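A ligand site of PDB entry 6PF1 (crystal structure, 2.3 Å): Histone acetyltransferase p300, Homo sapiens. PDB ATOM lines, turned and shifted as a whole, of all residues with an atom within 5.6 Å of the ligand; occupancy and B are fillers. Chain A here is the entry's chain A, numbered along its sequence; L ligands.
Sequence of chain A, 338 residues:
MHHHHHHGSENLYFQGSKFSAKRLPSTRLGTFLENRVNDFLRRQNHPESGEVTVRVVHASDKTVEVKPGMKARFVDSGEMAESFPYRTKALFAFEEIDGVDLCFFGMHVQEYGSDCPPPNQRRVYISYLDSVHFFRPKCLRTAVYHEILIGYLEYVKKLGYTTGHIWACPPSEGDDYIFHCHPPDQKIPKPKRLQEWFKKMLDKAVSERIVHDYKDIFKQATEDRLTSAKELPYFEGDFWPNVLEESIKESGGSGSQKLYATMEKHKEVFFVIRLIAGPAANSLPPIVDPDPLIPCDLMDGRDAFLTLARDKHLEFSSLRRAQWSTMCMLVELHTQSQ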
ATOM      1  N   ARG A 123     -11.244   0.575  -9.500  1.00  0.00           N
ATOM      2  CA  ARG A 123      -9.821   0.262  -9.578  1.00  0.00           C
ATOM      3  C   ARG A 123      -9.617  -1.067 -10.225  1.00  0.00           C
ATOM      4  O   ARG A 123     -10.396  -2.000  -9.981  1.00  0.00           O
ATOM      5  CB  ARG A 123      -9.254   0.174  -8.190  1.00  0.00           C
ATOM      6  CG  ARG A 123      -8.998   1.503  -7.517  1.00  0.00           C
ATOM      7  CD  ARG A 123      -8.416   1.276  -6.147  1.00  0.00           C
ATOM      8  NE  ARG A 123      -8.719   2.394  -5.274  1.00  0.00           N
ATOM      9  CZ  ARG A 123      -8.072   3.565  -5.250  1.00  0.00           C
ATOM     10  NH1 ARG A 123      -7.030   3.833  -6.052  1.00  0.00           N
ATOM     11  NH2 ARG A 123      -8.479   4.470  -4.366  1.00  0.00           N
ATOM     12  N   TYR A 125      -6.407  -4.046 -10.572  1.00  0.00           N
ATOM     13  CA  TYR A 125      -5.160  -4.503  -9.987  1.00  0.00           C
ATOM     14  C   TYR A 125      -4.707  -5.663 -10.846  1.00  0.00           C
ATOM     15  O   TYR A 125      -5.482  -6.556 -11.083  1.00  0.00           O
ATOM     16  CB  TYR A 125      -5.423  -4.985  -8.558  1.00  0.00           C
ATOM     17  CG  TYR A 125      -4.242  -5.685  -7.887  1.00  0.00           C
ATOM     18  CD1 TYR A 125      -2.961  -5.147  -7.934  1.00  0.00           C
ATOM     19  CD2 TYR A 125      -4.415  -6.872  -7.190  1.00  0.00           C
ATOM     20  CE1 TYR A 125      -1.895  -5.754  -7.291  1.00  0.00           C
ATOM     21  CE2 TYR A 125      -3.349  -7.500  -6.536  1.00  0.00           C
ATOM     22  CZ  TYR A 125      -2.089  -6.921  -6.584  1.00  0.00           C
ATOM     23  OH  TYR A 125      -1.009  -7.528  -5.942  1.00  0.00           O
ATOM     24  N   HIS A 165      -3.375  -0.443 -10.776  1.00  0.00           N
ATOM     25  CA  HIS A 165      -2.375  -0.733  -9.765  1.00  0.00           C
ATOM     26  C   HIS A 165      -1.511  -1.897 -10.242  1.00  0.00           C
ATOM     27  O   HIS A 165      -2.003  -2.959 -10.562  1.00  0.00           O
ATOM     28  CB  HIS A 165      -3.038  -1.064  -8.437  1.00  0.00           C
ATOM     29  CG  HIS A 165      -3.778   0.085  -7.829  1.00  0.00           C
ATOM     30  ND1 HIS A 165      -3.249   0.860  -6.825  1.00  0.00           N
ATOM     31  CD2 HIS A 165      -4.992   0.617  -8.121  1.00  0.00           C
ATOM     32  CE1 HIS A 165      -4.093   1.835  -6.521  1.00  0.00           C
ATOM     33  NE2 HIS A 165      -5.168   1.701  -7.284  1.00  0.00           N
ATOM     34  N   ILE A 166      -0.214  -1.668 -10.313  1.00  0.00           N
ATOM     35  CA  ILE A 166       0.699  -2.696 -10.753  1.00  0.00           C
ATOM     36  C   ILE A 166       1.755  -2.842  -9.682  1.00  0.00           C
ATOM     37  O   ILE A 166       2.259  -1.863  -9.180  1.00  0.00           O
ATOM     38  CB  ILE A 166       1.290  -2.311 -12.115  1.00  0.00           C
ATOM     39  CG1 ILE A 166       0.194  -2.408 -13.172  1.00  0.00           C
ATOM     40  CG2 ILE A 166       2.450  -3.201 -12.507  1.00  0.00           C
ATOM     41  CD1 ILE A 166       0.672  -2.259 -14.589  1.00  0.00           C
ATOM     42  N   TRP A 167       2.057  -4.091  -9.345  1.00  0.00           N
ATOM     43  CA  TRP A 167       3.140  -4.496  -8.464  1.00  0.00           C
ATOM     44  C   TRP A 167       4.195  -5.160  -9.389  1.00  0.00           C
ATOM     45  O   TRP A 167       3.900  -6.147 -10.054  1.00  0.00           O
ATOM     46  CB  TRP A 167       2.570  -5.467  -7.410  1.00  0.00           C
ATOM     47  CG  TRP A 167       3.536  -6.017  -6.424  1.00  0.00           C
ATOM     48  CD1 TRP A 167       4.795  -5.599  -6.228  1.00  0.00           C
ATOM     49  CD2 TRP A 167       3.311  -7.086  -5.454  1.00  0.00           C
ATOM     50  NE1 TRP A 167       5.395  -6.314  -5.226  1.00  0.00           N
ATOM     51  CE2 TRP A 167       4.516  -7.248  -4.731  1.00  0.00           C
ATOM     52  CE3 TRP A 167       2.215  -7.908  -5.140  1.00  0.00           C
ATOM     53  CZ2 TRP A 167       4.673  -8.210  -3.713  1.00  0.00           C
ATOM     54  CZ3 TRP A 167       2.372  -8.880  -4.124  1.00  0.00           C
ATOM     55  CH2 TRP A 167       3.590  -9.009  -3.425  1.00  0.00           C
ATOM     56  N   ILE A 217       3.812   4.867  -5.277  1.00  0.00           N
ATOM     57  CA  ILE A 217       2.930   4.967  -4.105  1.00  0.00           C
ATOM     58  C   ILE A 217       3.295   6.032  -3.083  1.00  0.00           C
ATOM     59  O   ILE A 217       2.399   6.528  -2.417  1.00  0.00           O
ATOM     60  CB  ILE A 217       2.795   3.626  -3.378  1.00  0.00           C
ATOM     61  CG1 ILE A 217       4.170   2.995  -3.166  1.00  0.00           C
ATOM     62  CG2 ILE A 217       1.889   2.712  -4.177  1.00  0.00           C
ATOM     63  CD1 ILE A 217       4.180   1.864  -2.173  1.00  0.00           C
ATOM     64  N   PHE A 218       4.589   6.357  -2.950  1.00  0.00           N
ATOM     65  CA  PHE A 218       5.053   7.344  -1.953  1.00  0.00           C
ATOM     66  C   PHE A 218       4.698   8.772  -2.431  1.00  0.00           C
ATOM     67  O   PHE A 218       4.062   9.527  -1.732  1.00  0.00           O
ATOM     68  CB  PHE A 218       6.548   7.149  -1.597  1.00  0.00           C
ATOM     69  CG  PHE A 218       7.089   8.160  -0.621  1.00  0.00           C
ATOM     70  CD1 PHE A 218       6.764   8.080   0.730  1.00  0.00           C
ATOM     71  CD2 PHE A 218       7.898   9.217  -1.056  1.00  0.00           C
ATOM     72  CE1 PHE A 218       7.227   9.039   1.638  1.00  0.00           C
ATOM     73  CE2 PHE A 218       8.360  10.185  -0.148  1.00  0.00           C
ATOM     74  CZ  PHE A 218       8.021  10.096   1.203  1.00  0.00           C
ATOM     75  N   GLN A 220       2.349   9.450  -4.526  1.00  0.00           N
ATOM     76  CA  GLN A 220       0.891   9.496  -4.574  1.00  0.00           C
ATOM     77  C   GLN A 220       0.288   9.725  -3.200  1.00  0.00           C
ATOM     78  O   GLN A 220      -0.608  10.566  -3.047  1.00  0.00           O
ATOM     79  CB  GLN A 220       0.310   8.207  -5.178  1.00  0.00           C
ATOM     80  CG  GLN A 220      -1.188   8.242  -5.461  1.00  0.00           C
ATOM     81  CD  GLN A 220      -1.518   9.115  -6.657  1.00  0.00           C
ATOM     82  OE1 GLN A 220      -0.959   8.921  -7.748  1.00  0.00           O
ATOM     83  NE2 GLN A 220      -2.421  10.073  -6.468  1.00  0.00           N
ATOM     84  N   ALA A 221       0.775   8.980  -2.212  1.00  0.00           N
ATOM     85  CA  ALA A 221       0.342   9.167  -0.819  1.00  0.00           C
ATOM     86  C   ALA A 221       0.636  10.580  -0.336  1.00  0.00           C
ATOM     87  O   ALA A 221      -0.249  11.211   0.218  1.00  0.00           O
ATOM     88  CB  ALA A 221       1.028   8.172   0.090  1.00  0.00           C
ATOM     89  N   ASP A 224      -1.769  12.921  -2.031  1.00  0.00           N
ATOM     90  CA  ASP A 224      -3.099  12.692  -1.474  1.00  0.00           C
ATOM     91  C   ASP A 224      -3.235  13.092  -0.003  1.00  0.00           C
ATOM     92  O   ASP A 224      -4.356  13.092   0.506  1.00  0.00           O
ATOM     93  CB  ASP A 224      -3.499  11.208  -1.636  1.00  0.00           C
ATOM     94  CG  ASP A 224      -3.738  10.795  -3.107  1.00  0.00           C
ATOM     95  OD1 ASP A 224      -3.849  11.688  -3.977  1.00  0.00           O
ATOM     96  OD2 ASP A 224      -3.810   9.568  -3.379  1.00  0.00           O
ATOM     97  N   LEU A 226      -2.401  11.438   2.652  1.00  0.00           N
ATOM     98  CA  LEU A 226      -2.957  10.248   3.272  1.00  0.00           C
ATOM     99  C   LEU A 226      -2.438  10.195   4.701  1.00  0.00           C
ATOM    100  O   LEU A 226      -1.269  10.485   4.947  1.00  0.00           O
ATOM    101  CB  LEU A 226      -2.530   9.007   2.503  1.00  0.00           C
ATOM    102  CG  LEU A 226      -2.701   7.633   3.163  1.00  0.00           C
ATOM    103  CD1 LEU A 226      -2.976   6.598   2.078  1.00  0.00           C
ATOM    104  CD2 LEU A 226      -1.533   7.196   4.066  1.00  0.00           C
ATOM    105  N   GLU A 231      -7.225   4.205   4.154  1.00  0.00           N
ATOM    106  CA  GLU A 231      -7.194   4.842   2.843  1.00  0.00           C
ATOM    107  C   GLU A 231      -6.481   4.023   1.764  1.00  0.00           C
ATOM    108  O   GLU A 231      -6.628   4.338   0.601  1.00  0.00           O
ATOM    109  CB  GLU A 231      -6.541   6.259   2.905  1.00  0.00           C
ATOM    110  CG  GLU A 231      -7.313   7.326   3.682  1.00  0.00           C
ATOM    111  CD  GLU A 231      -6.516   8.634   3.827  1.00  0.00           C
ATOM    112  OE1 GLU A 231      -5.853   8.831   4.870  1.00  0.00           O
ATOM    113  OE2 GLU A 231      -6.536   9.457   2.882  1.00  0.00           O
ATOM    114  N   LEU A 232      -5.707   2.996   2.125  1.00  0.00           N
ATOM    115  CA  LEU A 232      -5.055   2.158   1.123  1.00  0.00           C
ATOM    116  C   LEU A 232      -6.006   1.128   0.517  1.00  0.00           C
ATOM    117  O   LEU A 232      -6.769   0.467   1.257  1.00  0.00           O
ATOM    118  CB  LEU A 232      -3.918   1.374   1.728  1.00  0.00           C
ATOM    119  CG  LEU A 232      -2.726   2.153   2.255  1.00  0.00           C
ATOM    120  CD1 LEU A 232      -1.721   1.152   2.828  1.00  0.00           C
ATOM    121  CD2 LEU A 232      -2.134   2.962   1.130  1.00  0.00           C
ATOM    122  N   PRO A 233      -5.919   0.964  -0.831  1.00  0.00           N
ATOM    123  CA  PRO A 233      -6.667  -0.051  -1.546  1.00  0.00           C
ATOM    124  C   PRO A 233      -6.304  -1.445  -1.015  1.00  0.00           C
ATOM    125  O   PRO A 233      -5.101  -1.717  -0.783  1.00  0.00           O
ATOM    126  CB  PRO A 233      -6.217   0.102  -2.991  1.00  0.00           C
ATOM    127  CG  PRO A 233      -5.538   1.388  -3.089  1.00  0.00           C
ATOM    128  CD  PRO A 233      -5.011   1.696  -1.729  1.00  0.00           C
ATOM    129  N   TYR A 234      -7.325  -2.271  -0.824  1.00  0.00           N
ATOM    130  CA  TYR A 234      -7.236  -3.520  -0.176  1.00  0.00           C
ATOM    131  C   TYR A 234      -7.579  -4.595  -1.193  1.00  0.00           C
ATOM    132  O   TYR A 234      -8.744  -4.806  -1.507  1.00  0.00           O
ATOM    133  CB  TYR A 234      -8.223  -3.581   0.986  1.00  0.00           C
ATOM    134  CG  TYR A 234      -7.810  -4.585   2.035  1.00  0.00           C
ATOM    135  CD1 TYR A 234      -8.125  -5.921   1.904  1.00  0.00           C
ATOM    136  CD2 TYR A 234      -7.055  -4.183   3.137  1.00  0.00           C
ATOM    137  CE1 TYR A 234      -7.714  -6.857   2.891  1.00  0.00           C
ATOM    138  CE2 TYR A 234      -6.652  -5.077   4.108  1.00  0.00           C
ATOM    139  CZ  TYR A 234      -6.981  -6.415   3.992  1.00  0.00           C
ATOM    140  OH  TYR A 234      -6.536  -7.259   4.967  1.00  0.00           O
ATOM    141  N   PHE A 235      -6.543  -5.274  -1.678  1.00  0.00           N
ATOM    142  CA  PHE A 235      -6.642  -6.238  -2.765  1.00  0.00           C
ATOM    143  C   PHE A 235      -6.336  -7.673  -2.308  1.00  0.00           C
ATOM    144  O   PHE A 235      -5.551  -7.897  -1.355  1.00  0.00           O
ATOM    145  CB  PHE A 235      -5.629  -5.879  -3.890  1.00  0.00           C
ATOM    146  CG  PHE A 235      -5.760  -4.497  -4.478  1.00  0.00           C
ATOM    147  CD1 PHE A 235      -6.987  -3.929  -4.737  1.00  0.00           C
ATOM    148  CD2 PHE A 235      -4.622  -3.803  -4.894  1.00  0.00           C
ATOM    149  CE1 PHE A 235      -7.082  -2.678  -5.320  1.00  0.00           C
ATOM    150  CE2 PHE A 235      -4.717  -2.542  -5.476  1.00  0.00           C
ATOM    151  CZ  PHE A 235      -5.950  -1.980  -5.686  1.00  0.00           C
ATOM    152  N   ASP A 238      -2.366  -9.338  -2.238  1.00  0.00           N
ATOM    153  CA  ASP A 238      -1.396  -8.261  -2.418  1.00  0.00           C
ATOM    154  C   ASP A 238      -0.439  -8.142  -1.213  1.00  0.00           C
ATOM    155  O   ASP A 238      -0.765  -8.565  -0.103  1.00  0.00           O
ATOM    156  CB  ASP A 238      -2.169  -6.934  -2.600  1.00  0.00           C
ATOM    157  CG  ASP A 238      -1.259  -5.744  -2.878  1.00  0.00           C
ATOM    158  OD1 ASP A 238      -0.328  -5.828  -3.693  1.00  0.00           O
ATOM    159  OD2 ASP A 238      -1.475  -4.705  -2.252  1.00  0.00           O
ATOM    160  N   TRP A 240       0.379  -5.469   0.513  1.00  0.00           N
ATOM    161  CA  TRP A 240       0.036  -4.444   1.489  1.00  0.00           C
ATOM    162  C   TRP A 240      -0.885  -4.862   2.611  1.00  0.00           C
ATOM    163  O   TRP A 240      -0.668  -4.454   3.712  1.00  0.00           O
ATOM    164  CB  TRP A 240      -0.457  -3.165   0.817  1.00  0.00           C
ATOM    165  CG  TRP A 240       0.677  -2.516   0.196  1.00  0.00           C
ATOM    166  CD1 TRP A 240       1.040  -2.586  -1.082  1.00  0.00           C
ATOM    167  CD2 TRP A 240       1.696  -1.797   0.869  1.00  0.00           C
ATOM    168  NE1 TRP A 240       2.189  -1.907  -1.294  1.00  0.00           N
ATOM    169  CE2 TRP A 240       2.634  -1.408  -0.101  1.00  0.00           C
ATOM    170  CE3 TRP A 240       1.918  -1.447   2.204  1.00  0.00           C
ATOM    171  CZ2 TRP A 240       3.779  -0.672   0.207  1.00  0.00           C
ATOM    172  CZ3 TRP A 240       3.021  -0.693   2.516  1.00  0.00           C
ATOM    173  CH2 TRP A 240       3.952  -0.319   1.509  1.00  0.00           C
ATOM    174  N   PRO A 241      -1.908  -5.693   2.352  1.00  0.00           N
ATOM    175  CA  PRO A 241      -2.658  -6.270   3.466  1.00  0.00           C
ATOM    176  C   PRO A 241      -1.830  -7.180   4.425  1.00  0.00           C
ATOM    177  O   PRO A 241      -2.109  -7.201   5.633  1.00  0.00           O
ATOM    178  CB  PRO A 241      -3.733  -7.076   2.755  1.00  0.00           C
ATOM    179  CG  PRO A 241      -3.978  -6.327   1.499  1.00  0.00           C
ATOM    180  CD  PRO A 241      -2.626  -5.833   1.082  1.00  0.00           C
ATOM    181  N   MET A 263       6.188   2.698   2.569  1.00  0.00           N
ATOM    182  CA  MET A 263       5.901   3.098   1.199  1.00  0.00           C
ATOM    183  C   MET A 263       7.125   3.650   0.472  1.00  0.00           C
ATOM    184  O   MET A 263       7.454   3.173  -0.614  1.00  0.00           O
ATOM    185  CB  MET A 263       4.724   4.083   1.155  1.00  0.00           C
ATOM    186  CG  MET A 263       3.415   3.367   1.501  1.00  0.00           C
ATOM    187  SD  MET A 263       1.909   4.305   1.244  1.00  0.00           S
ATOM    188  CE  MET A 263       1.934   5.421   2.644  1.00  0.00           C
ATOM    189  N   PHE A 270       5.766  -0.222  -6.793  1.00  0.00           N
ATOM    190  CA  PHE A 270       4.300  -0.085  -6.837  1.00  0.00           C
ATOM    191  C   PHE A 270       3.862   1.164  -7.584  1.00  0.00           C
ATOM    192  O   PHE A 270       4.130   2.269  -7.139  1.00  0.00           O
ATOM    193  CB  PHE A 270       3.699  -0.062  -5.431  1.00  0.00           C
ATOM    194  CG  PHE A 270       3.926  -1.320  -4.623  1.00  0.00           C
ATOM    195  CD1 PHE A 270       3.022  -2.377  -4.685  1.00  0.00           C
ATOM    196  CD2 PHE A 270       4.985  -1.423  -3.739  1.00  0.00           C
ATOM    197  CE1 PHE A 270       3.204  -3.529  -3.919  1.00  0.00           C
ATOM    198  CE2 PHE A 270       5.160  -2.558  -2.951  1.00  0.00           C
ATOM    199  CZ  PHE A 270       4.277  -3.620  -3.049  1.00  0.00           C
ATOM    200  N   PHE A 271       3.127   0.953  -8.685  1.00  0.00           N
ATOM    201  CA  PHE A 271       2.675   2.036  -9.553  1.00  0.00           C
ATOM    202  C   PHE A 271       1.206   2.234  -9.367  1.00  0.00           C
ATOM    203  O   PHE A 271       0.458   1.278  -9.334  1.00  0.00           O
ATOM    204  CB  PHE A 271       2.952   1.694 -11.005  1.00  0.00           C
ATOM    205  CG  PHE A 271       4.412   1.460 -11.316  1.00  0.00           C
ATOM    206  CD1 PHE A 271       5.001   0.225 -11.076  1.00  0.00           C
ATOM    207  CD2 PHE A 271       5.183   2.454 -11.893  1.00  0.00           C
ATOM    208  CE1 PHE A 271       6.319  -0.008 -11.397  1.00  0.00           C
ATOM    209  CE2 PHE A 271       6.522   2.220 -12.208  1.00  0.00           C
ATOM    210  CZ  PHE A 271       7.090   0.984 -11.961  1.00  0.00           C
ATOM    211  N   VAL A 272       0.808   3.492  -9.210  1.00  0.00           N
ATOM    212  CA  VAL A 272      -0.575   3.935  -9.203  1.00  0.00           C
ATOM    213  C   VAL A 272      -0.842   4.698 -10.492  1.00  0.00           C
ATOM    214  O   VAL A 272      -0.192   5.750 -10.732  1.00  0.00           O
ATOM    215  CB  VAL A 272      -0.829   4.920  -8.063  1.00  0.00           C
ATOM    216  CG1 VAL A 272      -2.329   5.229  -7.949  1.00  0.00           C
ATOM    217  CG2 VAL A 272      -0.239   4.362  -6.784  1.00  0.00           C
HETATM  218  C1  LIG L   1      -0.640  -0.403  -4.708  1.00  0.00           C
HETATM  219  C2  LIG L   1      -0.524   2.172  -2.068  1.00  0.00           C
HETATM  220  C3  LIG L   1      -0.765  -1.792  -4.565  1.00  0.00           C
HETATM  221  C4  LIG L   1      -0.410  -2.683  -5.567  1.00  0.00           C
HETATM  222  C5  LIG L   1      -2.239   3.548  -3.669  1.00  0.00           C
HETATM  223  C6  LIG L   1       0.070  -2.151  -6.737  1.00  0.00           C
HETATM  224  C7  LIG L   1       0.224  -0.780  -6.898  1.00  0.00           C
HETATM  225  C8  LIG L   1      -0.139   0.102  -5.904  1.00  0.00           C
HETATM  226  C9  LIG L   1      -1.149   1.579  -3.168  1.00  0.00           C
HETATM  227  C10 LIG L   1      -1.608   4.219  -2.624  1.00  0.00           C
HETATM  228  C11 LIG L   1      -0.736   3.510  -1.818  1.00  0.00           C
HETATM  229  N1  LIG L   1      -1.275  -2.042  -3.316  1.00  0.00           N
HETATM  230  N2  LIG L   1      -2.028   2.253  -3.942  1.00  0.00           N
HETATM  231  C12 LIG L   1      -1.072   0.164  -3.460  1.00  0.00           C
HETATM  232  C13 LIG L   1      -2.007  -0.842  -1.255  1.00  0.00           C
HETATM  233  C14 LIG L   1      -1.462  -0.867  -2.645  1.00  0.00           C
HETATM  234 CL1  LIG L   1       0.580   1.288  -1.061  1.00  0.00          CL
HETATM  235  C15 LIG L   1      -1.863   5.654  -2.347  1.00  0.00           C
HETATM  236  F1  LIG L   1      -0.735   6.319  -2.204  1.00  0.00           F
HETATM  237  F2  LIG L   1      -2.540   6.283  -3.309  1.00  0.00           F
HETATM  238  F3  LIG L   1      -2.556   5.830  -1.205  1.00  0.00           F
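N1 of the ligand sits at hydrogen-bond distance from OD2 of Asp 238, 2.9 Å away. ND1 of His 165 lies close to N2 of the ligand (3.4 Å).
The backbone NH of Trp 240 sits close to the side-chain carboxylate of Asp 238 (3.4 Å). OH of Tyr 125 lies within hydrogen-bond range of OD1 of Asp 238 (2.9 Å). The backbone NH of Leu 226 sits at hydrogen-bond distance from the backbone carbonyl oxygen of Ala 221, at 3.3 Å. O of Phe 270 sits at hydrogen-bond distance from N of Ile 217 (3.2 Å). The backbone carbonyl oxygen of Ile 166 sits at hydrogen-bond distance from the backbone NH of Phe 271. The side-chain amide nitrogen (NE2) of Gln 220 lies within hydrogen-bond range of the side-chain carboxylate (OD1) of Asp 224 (3.3 Å). A ring nitrogen (NE2) of His 165 is in hydrogen-bond range of the guanidinium group of Arg 123 (3.1 Å).
A fluorine (F1) of the ligand lies close to the backbone carbonyl oxygen (O) of Ile 217. The backbone NH (N) of Ala 221 lies close to a fluorine (F1) of the ligand, at 3.1 Å. Merely in contact with the ligand: Tyr 125, Ile 166, Trp 167, Gln 220, Asp 224, Leu 226, Leu 232, Pro 233, Trp 240, Phe 270, Phe 271 and Val 272. Hydrophobic or aromatic side chains that line the ligand: Tyr 125, His 165, Ile 217, Ala 221, Leu 226, Leu 232, Pro 233, Trp 240, Phe 270 and Val 272. Of the 23 residues printed, 16 come within 4 Å of the ligand. Along chain A the residues within 4 Å of the ligand span positions 125 to 272. The nearest printed residue that does not touch the ligand is Met 263 (4.02 Å).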
